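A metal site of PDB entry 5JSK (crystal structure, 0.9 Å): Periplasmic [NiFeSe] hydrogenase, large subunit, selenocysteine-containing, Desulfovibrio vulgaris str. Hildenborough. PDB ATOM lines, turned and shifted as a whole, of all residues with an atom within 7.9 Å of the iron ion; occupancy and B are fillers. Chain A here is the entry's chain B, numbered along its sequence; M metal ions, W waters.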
ATOM      1  N   GLU A  53     -16.540  -2.324  17.522  1.00  0.00           N
ATOM      2  CA  GLU A  53     -16.678  -3.584  16.796  1.00  0.00           C
ATOM      3  C   GLU A  53     -17.922  -4.358  17.208  1.00  0.00           C
ATOM      4  O   GLU A  53     -18.432  -5.150  16.420  1.00  0.00           O
ATOM      5  CB  GLU A  53     -15.415  -4.416  16.979  1.00  0.00           C
ATOM      6  CG  GLU A  53     -14.215  -3.772  16.277  1.00  0.00           C
ATOM      7  CD  GLU A  53     -12.858  -4.129  16.868  1.00  0.00           C
ATOM      8  OE1 GLU A  53     -12.812  -4.414  18.086  1.00  0.00           O
ATOM      9  OE2 GLU A  53     -11.854  -4.059  16.109  1.00  0.00           O
ATOM     10  N   GLU A 279      -3.823 -10.686  16.352  1.00  0.00           N
ATOM     11  CA  GLU A 279      -3.973  -9.820  17.512  1.00  0.00           C
ATOM     12  C   GLU A 279      -4.006 -10.663  18.782  1.00  0.00           C
ATOM     13  O   GLU A 279      -4.882 -11.519  18.962  1.00  0.00           O
ATOM     14  CB  GLU A 279      -5.229  -8.959  17.415  1.00  0.00           C
ATOM     15  CG  GLU A 279      -5.164  -7.949  16.288  1.00  0.00           C
ATOM     16  CD  GLU A 279      -6.313  -6.964  16.339  1.00  0.00           C
ATOM     17  OE1 GLU A 279      -7.410  -7.313  15.867  1.00  0.00           O
ATOM     18  OE2 GLU A 279      -6.100  -5.857  16.887  1.00  0.00           O
ATOM     19  N   PHE A 286      -9.311  -8.388  27.361  1.00  0.00           N
ATOM     20  CA  PHE A 286     -10.218  -9.164  26.513  1.00  0.00           C
ATOM     21  C   PHE A 286     -10.135 -10.629  26.896  1.00  0.00           C
ATOM     22  O   PHE A 286      -9.137 -11.098  27.451  1.00  0.00           O
ATOM     23  CB  PHE A 286      -9.905  -8.973  25.018  1.00  0.00           C
ATOM     24  CG  PHE A 286     -10.032  -7.540  24.611  1.00  0.00           C
ATOM     25  CD1 PHE A 286     -11.264  -6.990  24.392  1.00  0.00           C
ATOM     26  CD2 PHE A 286      -8.915  -6.730  24.551  1.00  0.00           C
ATOM     27  CE1 PHE A 286     -11.397  -5.645  24.109  1.00  0.00           C
ATOM     28  CE2 PHE A 286      -9.043  -5.383  24.260  1.00  0.00           C
ATOM     29  CZ  PHE A 286     -10.283  -4.844  24.046  1.00  0.00           C
ATOM     30  N   TYR A 295      -7.647 -10.714  11.782  1.00  0.00           N
ATOM     31  CA  TYR A 295      -8.806  -9.823  11.820  1.00  0.00           C
ATOM     32  C   TYR A 295     -10.021 -10.403  11.083  1.00  0.00           C
ATOM     33  O   TYR A 295     -11.143 -10.057  11.440  1.00  0.00           O
ATOM     34  CB  TYR A 295      -8.418  -8.423  11.293  1.00  0.00           C
ATOM     35  CG  TYR A 295      -7.889  -8.482   9.883  1.00  0.00           C
ATOM     36  CD1 TYR A 295      -8.757  -8.511   8.797  1.00  0.00           C
ATOM     37  CD2 TYR A 295      -6.531  -8.577   9.630  1.00  0.00           C
ATOM     38  CE1 TYR A 295      -8.289  -8.625   7.506  1.00  0.00           C
ATOM     39  CE2 TYR A 295      -6.054  -8.703   8.356  1.00  0.00           C
ATOM     40  CZ  TYR A 295      -6.925  -8.739   7.290  1.00  0.00           C
ATOM     41  OH  TYR A 295      -6.422  -8.885   6.017  1.00  0.00           O
ATOM     42  N   GLY A 298     -11.673 -12.005  13.766  1.00  0.00           N
ATOM     43  CA  GLY A 298     -11.455 -11.314  15.008  1.00  0.00           C
ATOM     44  C   GLY A 298     -12.690 -11.304  15.895  1.00  0.00           C
ATOM     45  O   GLY A 298     -13.822 -11.432  15.444  1.00  0.00           O
ATOM     46  N   LYS A 299     -12.429 -11.121  17.186  1.00  0.00           N
ATOM     47  CA  LYS A 299     -13.463 -11.095  18.215  1.00  0.00           C
ATOM     48  C   LYS A 299     -13.092 -10.036  19.233  1.00  0.00           C
ATOM     49  O   LYS A 299     -11.908  -9.842  19.523  1.00  0.00           O
ATOM     50  CB  LYS A 299     -13.580 -12.437  18.942  1.00  0.00           C
ATOM     51  CG  LYS A 299     -14.064 -13.561  18.055  1.00  0.00           C
ATOM     52  CD  LYS A 299     -14.328 -14.833  18.842  1.00  0.00           C
ATOM     53  CE  LYS A 299     -15.069 -15.872  18.017  1.00  0.00           C
ATOM     54  NZ  LYS A 299     -16.457 -15.434  17.704  1.00  0.00           N
ATOM     55  N   THR A 300     -14.106  -9.375  19.779  1.00  0.00           N
ATOM     56  CA  THR A 300     -13.902  -8.309  20.756  1.00  0.00           C
ATOM     57  C   THR A 300     -14.827  -8.561  21.939  1.00  0.00           C
ATOM     58  O   THR A 300     -16.022  -8.225  21.886  1.00  0.00           O
ATOM     59  CB  THR A 300     -14.111  -6.966  20.101  1.00  0.00           C
ATOM     60  OG1 THR A 300     -13.246  -6.943  18.965  1.00  0.00           O
ATOM     61  CG2 THR A 300     -13.813  -5.837  21.070  1.00  0.00           C
ATOM     62  N   PHE A 312      -6.606  -1.679  27.165  1.00  0.00           N
ATOM     63  CA  PHE A 312      -7.685  -2.016  26.239  1.00  0.00           C
ATOM     64  C   PHE A 312      -7.225  -2.071  24.795  1.00  0.00           C
ATOM     65  O   PHE A 312      -8.029  -2.355  23.898  1.00  0.00           O
ATOM     66  CB  PHE A 312      -8.860  -1.044  26.368  1.00  0.00           C
ATOM     67  CG  PHE A 312      -9.664  -1.191  27.632  1.00  0.00           C
ATOM     68  CD1 PHE A 312     -10.429  -2.329  27.867  1.00  0.00           C
ATOM     69  CD2 PHE A 312      -9.689  -0.169  28.578  1.00  0.00           C
ATOM     70  CE1 PHE A 312     -11.176  -2.445  29.016  1.00  0.00           C
ATOM     71  CE2 PHE A 312     -10.449  -0.282  29.731  1.00  0.00           C
ATOM     72  CZ  PHE A 312     -11.184  -1.417  29.962  1.00  0.00           C
ATOM     73  N   LYS A 314      -5.407  -4.143  21.973  1.00  0.00           N
ATOM     74  CA  LYS A 314      -4.905  -5.478  21.637  1.00  0.00           C
ATOM     75  C   LYS A 314      -3.438  -5.375  21.217  1.00  0.00           C
ATOM     76  O   LYS A 314      -2.911  -4.275  21.019  1.00  0.00           O
ATOM     77  CB  LYS A 314      -5.762  -6.111  20.532  1.00  0.00           C
ATOM     78  CG  LYS A 314      -7.220  -6.377  20.901  1.00  0.00           C
ATOM     79  CD  LYS A 314      -7.977  -7.015  19.728  1.00  0.00           C
ATOM     80  CE  LYS A 314      -9.434  -7.298  20.032  1.00  0.00           C
ATOM     81  NZ  LYS A 314     -10.205  -7.598  18.784  1.00  0.00           N
ATOM     82  N   LEU A 423      -6.691  -0.805   8.772  1.00  0.00           N
ATOM     83  CA  LEU A 423      -7.555  -1.654   7.975  1.00  0.00           C
ATOM     84  C   LEU A 423      -8.874  -1.836   8.715  1.00  0.00           C
ATOM     85  O   LEU A 423      -8.935  -1.851   9.952  1.00  0.00           O
ATOM     86  CB  LEU A 423      -6.930  -2.986   7.589  1.00  0.00           C
ATOM     87  CG  LEU A 423      -6.723  -3.952   8.740  1.00  0.00           C
ATOM     88  CD1 LEU A 423      -7.913  -4.873   8.948  1.00  0.00           C
ATOM     89  CD2 LEU A 423      -5.454  -4.773   8.559  1.00  0.00           C
ATOM     90  N   TYR A 436     -17.291  -6.831  12.300  1.00  0.00           N
ATOM     91  CA  TYR A 436     -16.557  -5.668  11.826  1.00  0.00           C
ATOM     92  C   TYR A 436     -15.316  -5.598  12.710  1.00  0.00           C
ATOM     93  O   TYR A 436     -15.456  -5.544  13.931  1.00  0.00           O
ATOM     94  CB  TYR A 436     -17.403  -4.394  11.925  1.00  0.00           C
ATOM     95  CG  TYR A 436     -16.931  -3.279  11.015  1.00  0.00           C
ATOM     96  CD1 TYR A 436     -15.776  -2.549  11.285  1.00  0.00           C
ATOM     97  CD2 TYR A 436     -17.664  -2.940   9.876  1.00  0.00           C
ATOM     98  CE1 TYR A 436     -15.371  -1.521  10.446  1.00  0.00           C
ATOM     99  CE2 TYR A 436     -17.272  -1.909   9.040  1.00  0.00           C
ATOM    100  CZ  TYR A 436     -16.124  -1.196   9.327  1.00  0.00           C
ATOM    101  OH  TYR A 436     -15.773  -0.188   8.471  1.00  0.00           O
ATOM    102  N   GLN A 437     -14.143  -5.650  12.117  1.00  0.00           N
ATOM    103  CA  GLN A 437     -12.899  -5.636  12.867  1.00  0.00           C
ATOM    104  C   GLN A 437     -12.004  -4.531  12.345  1.00  0.00           C
ATOM    105  O   GLN A 437     -11.840  -4.359  11.138  1.00  0.00           O
ATOM    106  CB  GLN A 437     -12.206  -6.999  12.830  1.00  0.00           C
ATOM    107  CG  GLN A 437     -12.930  -8.041  13.643  1.00  0.00           C
ATOM    108  CD  GLN A 437     -12.798  -7.792  15.141  1.00  0.00           C
ATOM    109  OE1 GLN A 437     -11.732  -7.460  15.626  1.00  0.00           O
ATOM    110  NE2 GLN A 437     -13.884  -7.959  15.873  1.00  0.00           N
ATOM    111  N   ILE A 438     -11.409  -3.793  13.291  1.00  0.00           N
ATOM    112  CA  ILE A 438     -10.578  -2.634  13.008  1.00  0.00           C
ATOM    113  C   ILE A 438      -9.183  -2.889  13.573  1.00  0.00           C
ATOM    114  O   ILE A 438      -9.038  -3.246  14.746  1.00  0.00           O
ATOM    115  CB  ILE A 438     -11.204  -1.371  13.600  1.00  0.00           C
ATOM    116  CG1 ILE A 438     -12.542  -1.116  12.890  1.00  0.00           C
ATOM    117  CG2 ILE A 438     -10.252  -0.177  13.506  1.00  0.00           C
ATOM    118  CD1 ILE A 438     -13.519  -0.359  13.654  1.00  0.00           C
ATOM    119  N   VAL A 439      -8.171  -2.668  12.752  1.00  0.00           N
ATOM    120  CA  VAL A 439      -6.771  -2.777  13.141  1.00  0.00           C
ATOM    121  C   VAL A 439      -6.171  -1.426  12.738  1.00  0.00           C
ATOM    122  O   VAL A 439      -5.982  -1.169  11.553  1.00  0.00           O
ATOM    123  CB  VAL A 439      -6.079  -3.961  12.449  1.00  0.00           C
ATOM    124  CG1 VAL A 439      -4.604  -4.075  12.816  1.00  0.00           C
ATOM    125  CG2 VAL A 439      -6.806  -5.262  12.788  1.00  0.00           C
ATOM    126  N   SER A 440      -5.933  -0.543  13.713  1.00  0.00           N
ATOM    127  CA  SER A 440      -5.644   0.870  13.465  1.00  0.00           C
ATOM    128  C   SER A 440      -4.168   1.225  13.732  1.00  0.00           C
ATOM    129  O   SER A 440      -3.369   0.420  14.191  1.00  0.00           O
ATOM    130  CB  SER A 440      -6.526   1.702  14.372  1.00  0.00           C
ATOM    131  OG  SER A 440      -6.188   1.351  15.692  1.00  0.00           O
ATOM    132  N   LEU A 443      -2.920   1.396  17.390  1.00  0.00           N
ATOM    133  CA  LEU A 443      -2.880   0.001  17.832  1.00  0.00           C
ATOM    134  C   LEU A 443      -1.505  -0.597  17.585  1.00  0.00           C
ATOM    135  O   LEU A 443      -0.942  -1.245  18.469  1.00  0.00           O
ATOM    136  CB  LEU A 443      -3.980  -0.770  17.123  1.00  0.00           C
ATOM    137  CG  LEU A 443      -3.897  -2.278  17.140  1.00  0.00           C
ATOM    138  CD1 LEU A 443      -4.176  -2.875  18.487  1.00  0.00           C
ATOM    139  CD2 LEU A 443      -4.827  -2.844  16.097  1.00  0.00           C
ATOM    140  N   CYS A 489      -8.311   5.806  18.561  1.00  0.00           N
ATOM    141  CA  CYS A 489      -8.035   4.875  17.474  1.00  0.00           C
ATOM    142  C   CYS A 489      -7.512   3.547  17.980  1.00  0.00           C
ATOM    143  O   CYS A 489      -7.899   2.485  17.469  1.00  0.00           O
ATOM    144  CB  CYS A 489      -7.021   5.443  16.493  1.00  0.00           C
ATOM    145  SG  CYS A 489      -7.766   6.565  15.335  1.00  0.00           S
ATOM    146  N   ALA A 490      -6.561   3.569  18.913  1.00  0.00           N
ATOM    147  CA  ALA A 490      -5.897   2.316  19.297  1.00  0.00           C
ATOM    148  C   ALA A 490      -6.872   1.312  19.883  1.00  0.00           C
ATOM    149  O   ALA A 490      -6.732   0.101  19.656  1.00  0.00           O
ATOM    150  CB  ALA A 490      -4.793   2.597  20.302  1.00  0.00           C
ATOM    151  N   VAL A 491      -7.839   1.781  20.668  1.00  0.00           N
ATOM    152  CA  VAL A 491      -8.777   0.914  21.382  1.00  0.00           C
ATOM    153  C   VAL A 491     -10.085   0.720  20.624  1.00  0.00           C
ATOM    154  O   VAL A 491     -10.631  -0.388  20.572  1.00  0.00           O
ATOM    155  CB  VAL A 491      -9.078   1.459  22.791  1.00  0.00           C
ATOM    156  CG1 VAL A 491     -10.104   0.546  23.472  1.00  0.00           C
ATOM    157  CG2 VAL A 491      -7.837   1.580  23.636  1.00  0.00           C
ATOM    158  N   HIS A 492     -10.655   1.814  20.112  1.00  0.00           N
ATOM    159  CA  HIS A 492     -11.960   1.799  19.491  1.00  0.00           C
ATOM    160  C   HIS A 492     -13.002   1.051  20.330  1.00  0.00           C
ATOM    161  O   HIS A 492     -13.079   1.345  21.558  1.00  0.00           O
ATOM    162  CB  HIS A 492     -11.892   1.364  17.993  1.00  0.00           C
ATOM    163  CG  HIS A 492     -11.005   0.188  17.697  1.00  0.00           C
ATOM    164  ND1 HIS A 492      -9.644   0.324  17.568  1.00  0.00           N
ATOM    165  CD2 HIS A 492     -11.273  -1.115  17.452  1.00  0.00           C
ATOM    166  CE1 HIS A 492      -9.110  -0.856  17.298  1.00  0.00           C
ATOM    167  NE2 HIS A 492     -10.080  -1.753  17.232  1.00  0.00           N
HETATM  168 FE    FE M   1      -9.751  -3.860  16.752  1.00  0.00          FE
HETATM  169  O   HOH W   1     -10.283  -4.437  18.842  1.00  0.00           O
HETATM  170  O   HOH W   2      -7.742  -3.865  17.435  1.00  0.00           O
HETATM  171  O   HOH W   3      -9.582  -5.931  16.292  1.00  0.00           O
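The side-chain carboxylate of Glu 53 sits close to the side-chain amide oxygen of Gln 437, 3.4 Å away.
A ring nitrogen (ND1) of His 492 lies within hydrogen-bond range of the backbone carbonyl oxygen (O) of Cys 489 (2.8 Å).
OG1 of Thr 300 sits at hydrogen-bond distance from OE1 of Glu 53 (2.7 Å).
Three residues have an atom within 4 Å of the iron ion: Glu 53, Ile 438 and His 492.
The nearest printed residue that does not touch the iron ion is Glu 279 (4.2 Å).
The iron ion is bound by water W2, water W3, a ring nitrogen (NE2) of His 492, the side-chain carboxylate of Glu 53, the backbone carbonyl oxygen of Ile 438 and water W1.
Water W3 lies within hydrogen-bond range of the side-chain carboxylate of Glu 279 (2.6 Å), the side-chain amide oxygen of Gln 437 (2.7 Å) and the side-chain amino group of Lys 314 (3.1 Å).
Water W1 lies within hydrogen-bond range of the side-chain carboxylate of Glu 53 (2.6 Å) and the side-chain amino group of Lys 314 (3.2 Å).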
